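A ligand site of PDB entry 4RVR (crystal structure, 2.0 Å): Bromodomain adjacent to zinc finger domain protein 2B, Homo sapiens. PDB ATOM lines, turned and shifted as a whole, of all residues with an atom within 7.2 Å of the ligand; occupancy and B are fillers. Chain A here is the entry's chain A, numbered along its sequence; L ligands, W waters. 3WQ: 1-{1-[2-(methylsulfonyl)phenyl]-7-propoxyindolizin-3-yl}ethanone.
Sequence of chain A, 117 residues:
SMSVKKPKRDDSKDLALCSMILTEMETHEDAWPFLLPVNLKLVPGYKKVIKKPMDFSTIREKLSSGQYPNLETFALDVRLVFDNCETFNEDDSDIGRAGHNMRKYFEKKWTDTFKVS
The backbone NH (N) of Asn 39 is in hydrogen-bond range of an oxygen (OAF) of the ligand, at 3.1 Å. The side-chain amide nitrogen (ND2) of Asn 89 is in hydrogen-bond range of an oxygen (OAD) of the ligand (3.2 Å).
The side-chain amide oxygen (OD1) of Asn 39 lies within hydrogen-bond range of the backbone NH (N) of Leu 42 (3.3 Å). The side-chain amide nitrogen (ND2) of Asn 89 is in hydrogen-bond range of the backbone carbonyl oxygen (O) of Cys 85 (3.0 Å). The backbone carbonyl oxygen of Ile 95 is in hydrogen-bond range of the side-chain sulfur of Cys 85 (3.6 Å).
Residues that only touch the ligand: Leu 36 (3.1 Å), Pro 33 (3.2 Å), Pro 37 (3.4 Å), Val 38 (3.4 Å), Leu 42 (3.5 Å), Val 43 (3.5 Å), Ile 95 (3.7 Å), Phe 34 (3.7 Å) and Trp 32 (3.8 Å). Hydrophobic or aromatic side chains that line the ligand: Trp 32, Pro 33, Phe 34, Val 38, Val 43 and Ile 95.
Water W3 lies within hydrogen-bond range of OH of Tyr 46, OAD of the ligand, N of Cys 85 and O of Asn 84.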
ATOM      1  N   TRP A  32     -15.208 -21.161 -10.413  1.00  0.00           N
ATOM      2  CA  TRP A  32     -16.172 -22.204 -10.079  1.00  0.00           C
ATOM      3  C   TRP A  32     -17.641 -21.878 -10.341  1.00  0.00           C
ATOM      4  O   TRP A  32     -18.398 -22.797 -10.715  1.00  0.00           O
ATOM      5  CB  TRP A  32     -15.957 -22.752  -8.645  1.00  0.00           C
ATOM      6  CG  TRP A  32     -16.053 -21.690  -7.575  1.00  0.00           C
ATOM      7  CD1 TRP A  32     -15.010 -20.991  -7.040  1.00  0.00           C
ATOM      8  CD2 TRP A  32     -17.247 -21.195  -6.943  1.00  0.00           C
ATOM      9  NE1 TRP A  32     -15.473 -20.103  -6.117  1.00  0.00           N
ATOM     10  CE2 TRP A  32     -16.839 -20.192  -6.037  1.00  0.00           C
ATOM     11  CE3 TRP A  32     -18.614 -21.481  -7.070  1.00  0.00           C
ATOM     12  CZ2 TRP A  32     -17.755 -19.462  -5.265  1.00  0.00           C
ATOM     13  CZ3 TRP A  32     -19.522 -20.809  -6.276  1.00  0.00           C
ATOM     14  CH2 TRP A  32     -19.080 -19.783  -5.378  1.00  0.00           C
ATOM     15  N   PRO A  33     -18.061 -20.605 -10.221  1.00  0.00           N
ATOM     16  CA  PRO A  33     -19.468 -20.380 -10.553  1.00  0.00           C
ATOM     17  C   PRO A  33     -19.788 -20.489 -12.042  1.00  0.00           C
ATOM     18  O   PRO A  33     -20.965 -20.452 -12.393  1.00  0.00           O
ATOM     19  CB  PRO A  33     -19.718 -18.937 -10.123  1.00  0.00           C
ATOM     20  CG  PRO A  33     -18.616 -18.602  -9.110  1.00  0.00           C
ATOM     21  CD  PRO A  33     -17.433 -19.367  -9.641  1.00  0.00           C
ATOM     22  N   PHE A  34     -18.738 -20.460 -12.899  1.00  0.00           N
ATOM     23  CA  PHE A  34     -18.855 -20.118 -14.347  1.00  0.00           C
ATOM     24  C   PHE A  34     -18.449 -21.253 -15.293  1.00  0.00           C
ATOM     25  O   PHE A  34     -18.458 -21.099 -16.493  1.00  0.00           O
ATOM     26  CB  PHE A  34     -18.033 -18.872 -14.667  1.00  0.00           C
ATOM     27  CG  PHE A  34     -18.268 -17.737 -13.706  1.00  0.00           C
ATOM     28  CD1 PHE A  34     -19.523 -17.131 -13.626  1.00  0.00           C
ATOM     29  CD2 PHE A  34     -17.259 -17.311 -12.854  1.00  0.00           C
ATOM     30  CE1 PHE A  34     -19.770 -16.131 -12.685  1.00  0.00           C
ATOM     31  CE2 PHE A  34     -17.503 -16.301 -11.935  1.00  0.00           C
ATOM     32  CZ  PHE A  34     -18.739 -15.699 -11.863  1.00  0.00           C
ATOM     33  N   LEU A  35     -18.118 -22.398 -14.719  1.00  0.00           N
ATOM     34  CA  LEU A  35     -17.646 -23.526 -15.479  1.00  0.00           C
ATOM     35  C   LEU A  35     -18.737 -24.223 -16.296  1.00  0.00           C
ATOM     36  O   LEU A  35     -18.460 -24.691 -17.361  1.00  0.00           O
ATOM     37  CB  LEU A  35     -16.942 -24.519 -14.573  1.00  0.00           C
ATOM     38  CG  LEU A  35     -15.696 -23.957 -13.851  1.00  0.00           C
ATOM     39  CD1 LEU A  35     -15.050 -25.070 -13.030  1.00  0.00           C
ATOM     40  CD2 LEU A  35     -14.695 -23.372 -14.846  1.00  0.00           C
ATOM     41  N   LEU A  36     -19.975 -24.247 -15.769  1.00  0.00           N
ATOM     42  CA  LEU A  36     -21.125 -24.885 -16.436  1.00  0.00           C
ATOM     43  C   LEU A  36     -22.265 -23.905 -16.494  1.00  0.00           C
ATOM     44  O   LEU A  36     -22.297 -22.905 -15.723  1.00  0.00           O
ATOM     45  CB  LEU A  36     -21.613 -26.120 -15.649  1.00  0.00           C
ATOM     46  CG  LEU A  36     -20.593 -27.226 -15.477  1.00  0.00           C
ATOM     47  CD1 LEU A  36     -21.154 -28.279 -14.498  1.00  0.00           C
ATOM     48  CD2 LEU A  36     -20.279 -27.812 -16.853  1.00  0.00           C
ATOM     49  N   PRO A  37     -23.263 -24.193 -17.356  1.00  0.00           N
ATOM     50  CA  PRO A  37     -24.434 -23.340 -17.348  1.00  0.00           C
ATOM     51  C   PRO A  37     -25.116 -23.334 -16.007  1.00  0.00           C
ATOM     52  O   PRO A  37     -25.054 -24.316 -15.283  1.00  0.00           O
ATOM     53  CB  PRO A  37     -25.357 -24.004 -18.388  1.00  0.00           C
ATOM     54  CG  PRO A  37     -24.500 -24.896 -19.200  1.00  0.00           C
ATOM     55  CD  PRO A  37     -23.396 -25.325 -18.306  1.00  0.00           C
ATOM     56  N   VAL A  38     -25.695 -22.194 -15.652  1.00  0.00           N
ATOM     57  CA  VAL A  38     -26.414 -22.117 -14.381  1.00  0.00           C
ATOM     58  C   VAL A  38     -27.576 -23.071 -14.471  1.00  0.00           C
ATOM     59  O   VAL A  38     -28.277 -23.138 -15.488  1.00  0.00           O
ATOM     60  CB  VAL A  38     -26.932 -20.724 -14.105  1.00  0.00           C
ATOM     61  CG1 VAL A  38     -27.901 -20.709 -12.881  1.00  0.00           C
ATOM     62  CG2 VAL A  38     -25.770 -19.766 -13.937  1.00  0.00           C
ATOM     63  N   ASN A  39     -27.713 -23.872 -13.431  1.00  0.00           N
ATOM     64  CA  ASN A  39     -28.660 -24.946 -13.473  1.00  0.00           C
ATOM     65  C   ASN A  39     -30.104 -24.442 -13.433  1.00  0.00           C
ATOM     66  O   ASN A  39     -30.599 -24.007 -12.374  1.00  0.00           O
ATOM     67  CB  ASN A  39     -28.366 -25.872 -12.311  1.00  0.00           C
ATOM     68  CG  ASN A  39     -29.223 -27.117 -12.348  1.00  0.00           C
ATOM     69  OD1 ASN A  39     -30.356 -27.125 -12.865  1.00  0.00           O
ATOM     70  ND2 ASN A  39     -28.686 -28.206 -11.806  1.00  0.00           N
ATOM     71  N   LEU A  40     -30.773 -24.453 -14.588  1.00  0.00           N
ATOM     72  CA  LEU A  40     -32.089 -23.803 -14.706  1.00  0.00           C
ATOM     73  C   LEU A  40     -33.192 -24.515 -13.928  1.00  0.00           C
ATOM     74  O   LEU A  40     -34.245 -23.916 -13.646  1.00  0.00           O
ATOM     75  CB  LEU A  40     -32.504 -23.672 -16.166  1.00  0.00           C
ATOM     76  CG  LEU A  40     -31.677 -22.746 -17.078  1.00  0.00           C
ATOM     77  CD1 LEU A  40     -32.404 -22.586 -18.403  1.00  0.00           C
ATOM     78  CD2 LEU A  40     -31.396 -21.381 -16.466  1.00  0.00           C
ATOM     79  N   LEU A  42     -32.685 -25.934 -10.904  1.00  0.00           N
ATOM     80  CA  LEU A  42     -32.440 -25.789  -9.479  1.00  0.00           C
ATOM     81  C   LEU A  42     -32.383 -24.361  -9.017  1.00  0.00           C
ATOM     82  O   LEU A  42     -32.371 -24.104  -7.814  1.00  0.00           O
ATOM     83  CB  LEU A  42     -31.107 -26.487  -9.109  1.00  0.00           C
ATOM     84  CG  LEU A  42     -31.160 -27.994  -8.875  1.00  0.00           C
ATOM     85  CD1 LEU A  42     -31.753 -28.741 -10.061  1.00  0.00           C
ATOM     86  CD2 LEU A  42     -29.766 -28.498  -8.527  1.00  0.00           C
ATOM     87  N   VAL A  43     -32.321 -23.416  -9.957  1.00  0.00           N
ATOM     88  CA  VAL A  43     -32.082 -22.019  -9.599  1.00  0.00           C
ATOM     89  C   VAL A  43     -33.304 -21.186  -9.978  1.00  0.00           C
ATOM     90  O   VAL A  43     -33.503 -20.889 -11.176  1.00  0.00           O
ATOM     91  CB  VAL A  43     -30.780 -21.437 -10.233  1.00  0.00           C
ATOM     92  CG1 VAL A  43     -30.524 -20.036  -9.726  1.00  0.00           C
ATOM     93  CG2 VAL A  43     -29.584 -22.339  -9.938  1.00  0.00           C
ATOM     94  N   PRO A  44     -34.158 -20.852  -8.974  1.00  0.00           N
ATOM     95  CA  PRO A  44     -35.383 -20.096  -9.270  1.00  0.00           C
ATOM     96  C   PRO A  44     -35.059 -18.671  -9.660  1.00  0.00           C
ATOM     97  O   PRO A  44     -34.150 -18.050  -9.065  1.00  0.00           O
ATOM     98  CB  PRO A  44     -36.147 -20.129  -7.924  1.00  0.00           C
ATOM     99  CG  PRO A  44     -35.091 -20.292  -6.896  1.00  0.00           C
ATOM    100  CD  PRO A  44     -34.039 -21.163  -7.536  1.00  0.00           C
ATOM    101  N   TYR A  46     -33.854 -17.765 -12.570  1.00  0.00           N
ATOM    102  CA  TYR A  46     -32.736 -17.577 -13.523  1.00  0.00           C
ATOM    103  C   TYR A  46     -33.204 -17.511 -14.948  1.00  0.00           C
ATOM    104  O   TYR A  46     -32.980 -16.507 -15.655  1.00  0.00           O
ATOM    105  CB  TYR A  46     -31.641 -18.666 -13.389  1.00  0.00           C
ATOM    106  CG  TYR A  46     -30.325 -18.098 -13.901  1.00  0.00           C
ATOM    107  CD1 TYR A  46     -29.955 -18.247 -15.240  1.00  0.00           C
ATOM    108  CD2 TYR A  46     -29.543 -17.293 -13.085  1.00  0.00           C
ATOM    109  CE1 TYR A  46     -28.766 -17.671 -15.742  1.00  0.00           C
ATOM    110  CE2 TYR A  46     -28.355 -16.692 -13.550  1.00  0.00           C
ATOM    111  CZ  TYR A  46     -27.974 -16.876 -14.871  1.00  0.00           C
ATOM    112  OH  TYR A  46     -26.796 -16.265 -15.338  1.00  0.00           O
ATOM    113  N   MET A  54     -24.926 -17.458 -20.260  1.00  0.00           N
ATOM    114  CA  MET A  54     -23.647 -17.846 -20.867  1.00  0.00           C
ATOM    115  C   MET A  54     -22.711 -18.313 -19.775  1.00  0.00           C
ATOM    116  O   MET A  54     -22.889 -17.916 -18.593  1.00  0.00           O
ATOM    117  CB  MET A  54     -23.083 -16.658 -21.662  1.00  0.00           C
ATOM    118  CG  MET A  54     -21.850 -16.964 -22.503  1.00  0.00           C
ATOM    119  SD  MET A  54     -22.005 -18.379 -23.642  1.00  0.00           S
ATOM    120  CE  MET A  54     -23.460 -17.821 -24.572  1.00  0.00           C
ATOM    121  N   ASP A  55     -21.807 -19.247 -20.129  1.00  0.00           N
ATOM    122  CA  ASP A  55     -20.828 -19.798 -19.188  1.00  0.00           C
ATOM    123  C   ASP A  55     -19.592 -20.205 -19.946  1.00  0.00           C
ATOM    124  O   ASP A  55     -19.611 -20.260 -21.208  1.00  0.00           O
ATOM    125  CB  ASP A  55     -21.392 -20.982 -18.424  1.00  0.00           C
ATOM    126  CG  ASP A  55     -21.510 -22.187 -19.304  1.00  0.00           C
ATOM    127  OD1 ASP A  55     -20.690 -23.084 -19.157  1.00  0.00           O
ATOM    128  OD2 ASP A  55     -22.391 -22.193 -20.173  1.00  0.00           O
ATOM    129  N   VAL A  81     -21.201 -13.297 -19.456  1.00  0.00           N
ATOM    130  CA  VAL A  81     -21.071 -14.125 -18.235  1.00  0.00           C
ATOM    131  C   VAL A  81     -21.054 -13.254 -16.958  1.00  0.00           C
ATOM    132  O   VAL A  81     -21.794 -13.515 -15.959  1.00  0.00           O
ATOM    133  CB  VAL A  81     -19.786 -15.002 -18.274  1.00  0.00           C
ATOM    134  CG1 VAL A  81     -19.668 -15.803 -16.957  1.00  0.00           C
ATOM    135  CG2 VAL A  81     -19.812 -16.002 -19.401  1.00  0.00           C
ATOM    136  N   ASN A  84     -24.430 -11.069 -16.586  1.00  0.00           N
ATOM    137  CA  ASN A  84     -25.425 -11.958 -15.943  1.00  0.00           C
ATOM    138  C   ASN A  84     -25.176 -12.142 -14.436  1.00  0.00           C
ATOM    139  O   ASN A  84     -26.091 -12.068 -13.619  1.00  0.00           O
ATOM    140  CB  ASN A  84     -25.490 -13.323 -16.618  1.00  0.00           C
ATOM    141  CG  ASN A  84     -25.953 -13.260 -18.084  1.00  0.00           C
ATOM    142  OD1 ASN A  84     -26.494 -12.248 -18.544  1.00  0.00           O
ATOM    143  ND2 ASN A  84     -25.814 -14.384 -18.800  1.00  0.00           N
ATOM    144  N   CYS A  85     -23.917 -12.365 -14.066  1.00  0.00           N
ATOM    145  CA  CYS A  85     -23.593 -12.655 -12.727  1.00  0.00           C
ATOM    146  C   CYS A  85     -24.008 -11.454 -11.808  1.00  0.00           C
ATOM    147  O   CYS A  85     -24.589 -11.638 -10.749  1.00  0.00           O
ATOM    148  CB  CYS A  85     -22.121 -13.004 -12.609  1.00  0.00           C
ATOM    149  SG  CYS A  85     -21.572 -13.363 -10.928  1.00  0.00           S
ATOM    150  N   GLU A  86     -23.762 -10.239 -12.289  1.00  0.00           N
ATOM    151  CA  GLU A  86     -24.074  -9.030 -11.553  1.00  0.00           C
ATOM    152  C   GLU A  86     -25.565  -8.784 -11.480  1.00  0.00           C
ATOM    153  O   GLU A  86     -26.068  -8.249 -10.487  1.00  0.00           O
ATOM    154  CB  GLU A  86     -23.423  -7.819 -12.250  1.00  0.00           C
ATOM    155  CG  GLU A  86     -21.966  -7.599 -11.924  1.00  0.00           C
ATOM    156  CD  GLU A  86     -21.541  -6.152 -12.130  1.00  0.00           C
ATOM    157  OE1 GLU A  86     -22.265  -5.237 -11.699  1.00  0.00           O
ATOM    158  OE2 GLU A  86     -20.452  -5.953 -12.700  1.00  0.00           O
ATOM    159  N   PHE A  88     -27.887 -11.154 -11.376  1.00  0.00           N
ATOM    160  CA  PHE A  88     -28.530 -12.131 -10.527  1.00  0.00           C
ATOM    161  C   PHE A  88     -28.020 -12.207  -9.104  1.00  0.00           C
ATOM    162  O   PHE A  88     -28.739 -12.685  -8.217  1.00  0.00           O
ATOM    163  CB  PHE A  88     -28.432 -13.525 -11.137  1.00  0.00           C
ATOM    164  CG  PHE A  88     -29.544 -14.448 -10.713  1.00  0.00           C
ATOM    165  CD1 PHE A  88     -30.800 -14.325 -11.270  1.00  0.00           C
ATOM    166  CD2 PHE A  88     -29.338 -15.452  -9.784  1.00  0.00           C
ATOM    167  CE1 PHE A  88     -31.846 -15.175 -10.907  1.00  0.00           C
ATOM    168  CE2 PHE A  88     -30.361 -16.308  -9.416  1.00  0.00           C
ATOM    169  CZ  PHE A  88     -31.623 -16.161  -9.972  1.00  0.00           C
ATOM    170  N   ASN A  89     -26.770 -11.852  -8.894  1.00  0.00           N
ATOM    171  CA  ASN A  89     -26.143 -12.060  -7.576  1.00  0.00           C
ATOM    172  C   ASN A  89     -25.782 -10.742  -6.880  1.00  0.00           C
ATOM    173  O   ASN A  89     -25.358  -9.783  -7.531  1.00  0.00           O
ATOM    174  CB  ASN A  89     -24.887 -12.846  -7.730  1.00  0.00           C
ATOM    175  CG  ASN A  89     -25.135 -14.237  -8.275  1.00  0.00           C
ATOM    176  OD1 ASN A  89     -25.373 -15.176  -7.525  1.00  0.00           O
ATOM    177  ND2 ASN A  89     -25.057 -14.384  -9.578  1.00  0.00           N
ATOM    178  N   ILE A  95     -20.427 -15.747  -4.988  1.00  0.00           N
ATOM    179  CA  ILE A  95     -20.537 -15.779  -6.458  1.00  0.00           C
ATOM    180  C   ILE A  95     -20.327 -14.383  -7.060  1.00  0.00           C
ATOM    181  O   ILE A  95     -19.575 -14.216  -8.039  1.00  0.00           O
ATOM    182  CB  ILE A  95     -21.892 -16.330  -6.914  1.00  0.00           C
ATOM    183  CG1 ILE A  95     -21.969 -17.816  -6.535  1.00  0.00           C
ATOM    184  CG2 ILE A  95     -22.079 -16.120  -8.445  1.00  0.00           C
ATOM    185  CD1 ILE A  95     -23.322 -18.449  -6.680  1.00  0.00           C
HETATM  186  CAA 3WQ L   1     -29.548 -24.189  -5.712  1.00  0.00           C
HETATM  187  CAO 3WQ L   1     -29.139 -22.720  -5.483  1.00  0.00           C
HETATM  188  CAP 3WQ L   1     -27.903 -22.382  -6.351  1.00  0.00           C
HETATM  189  OAQ 3WQ L   1     -28.047 -21.051  -6.902  1.00  0.00           O
HETATM  190  CAS 3WQ L   1     -27.111 -20.604  -7.805  1.00  0.00           C
HETATM  191  CAN 3WQ L   1     -25.949 -21.329  -8.165  1.00  0.00           C
HETATM  192  CAX 3WQ L   1     -25.072 -20.817  -9.054  1.00  0.00           C
HETATM  193  CAK 3WQ L   1     -27.344 -19.339  -8.355  1.00  0.00           C
HETATM  194  CAL 3WQ L   1     -26.432 -18.805  -9.252  1.00  0.00           C
HETATM  195  NAY 3WQ L   1     -25.306 -19.599  -9.584  1.00  0.00           N
HETATM  196  CAU 3WQ L   1     -24.285 -19.256 -10.419  1.00  0.00           C
HETATM  197  CAR 3WQ L   1     -24.235 -18.054 -11.132  1.00  0.00           C
HETATM  198  OAD 3WQ L   1     -25.121 -17.168 -11.088  1.00  0.00           O
HETATM  199  CAB 3WQ L   1     -23.040 -17.816 -12.055  1.00  0.00           C
HETATM  200  CAM 3WQ L   1     -23.419 -20.292 -10.414  1.00  0.00           C
HETATM  201  CAV 3WQ L   1     -23.897 -21.246  -9.549  1.00  0.00           C
HETATM  202  CAT 3WQ L   1     -23.277 -22.418  -9.194  1.00  0.00           C
HETATM  203  CAI 3WQ L   1     -22.513 -22.411  -8.021  1.00  0.00           C
HETATM  204  CAG 3WQ L   1     -21.791 -23.506  -7.561  1.00  0.00           C
HETATM  205  CAH 3WQ L   1     -21.776 -24.693  -8.285  1.00  0.00           C
HETATM  206  CAJ 3WQ L   1     -22.524 -24.733  -9.457  1.00  0.00           C
HETATM  207  CAW 3WQ L   1     -23.260 -23.630  -9.901  1.00  0.00           C
HETATM  208  SAZ 3WQ L   1     -24.123 -23.847 -11.435  1.00  0.00           S
HETATM  209  OAE 3WQ L   1     -24.099 -25.336 -11.617  1.00  0.00           O
HETATM  210  OAF 3WQ L   1     -25.487 -23.331 -11.313  1.00  0.00           O
HETATM  211  CAC 3WQ L   1     -23.190 -23.055 -12.725  1.00  0.00           C
HETATM  212  O   HOH W   1     -22.411 -20.414 -14.780  1.00  0.00           O
HETATM  213  O   HOH W   2     -24.939 -27.620 -12.791  1.00  0.00           O
HETATM  214  O   HOH W   3     -25.254 -15.458 -13.464  1.00  0.00           O
HETATM  215  O   HOH W   4     -23.092 -21.495  -4.700  1.00  0.00           O
HETATM  216  O   HOH W   5     -19.977 -23.986 -12.635  1.00  0.00           O
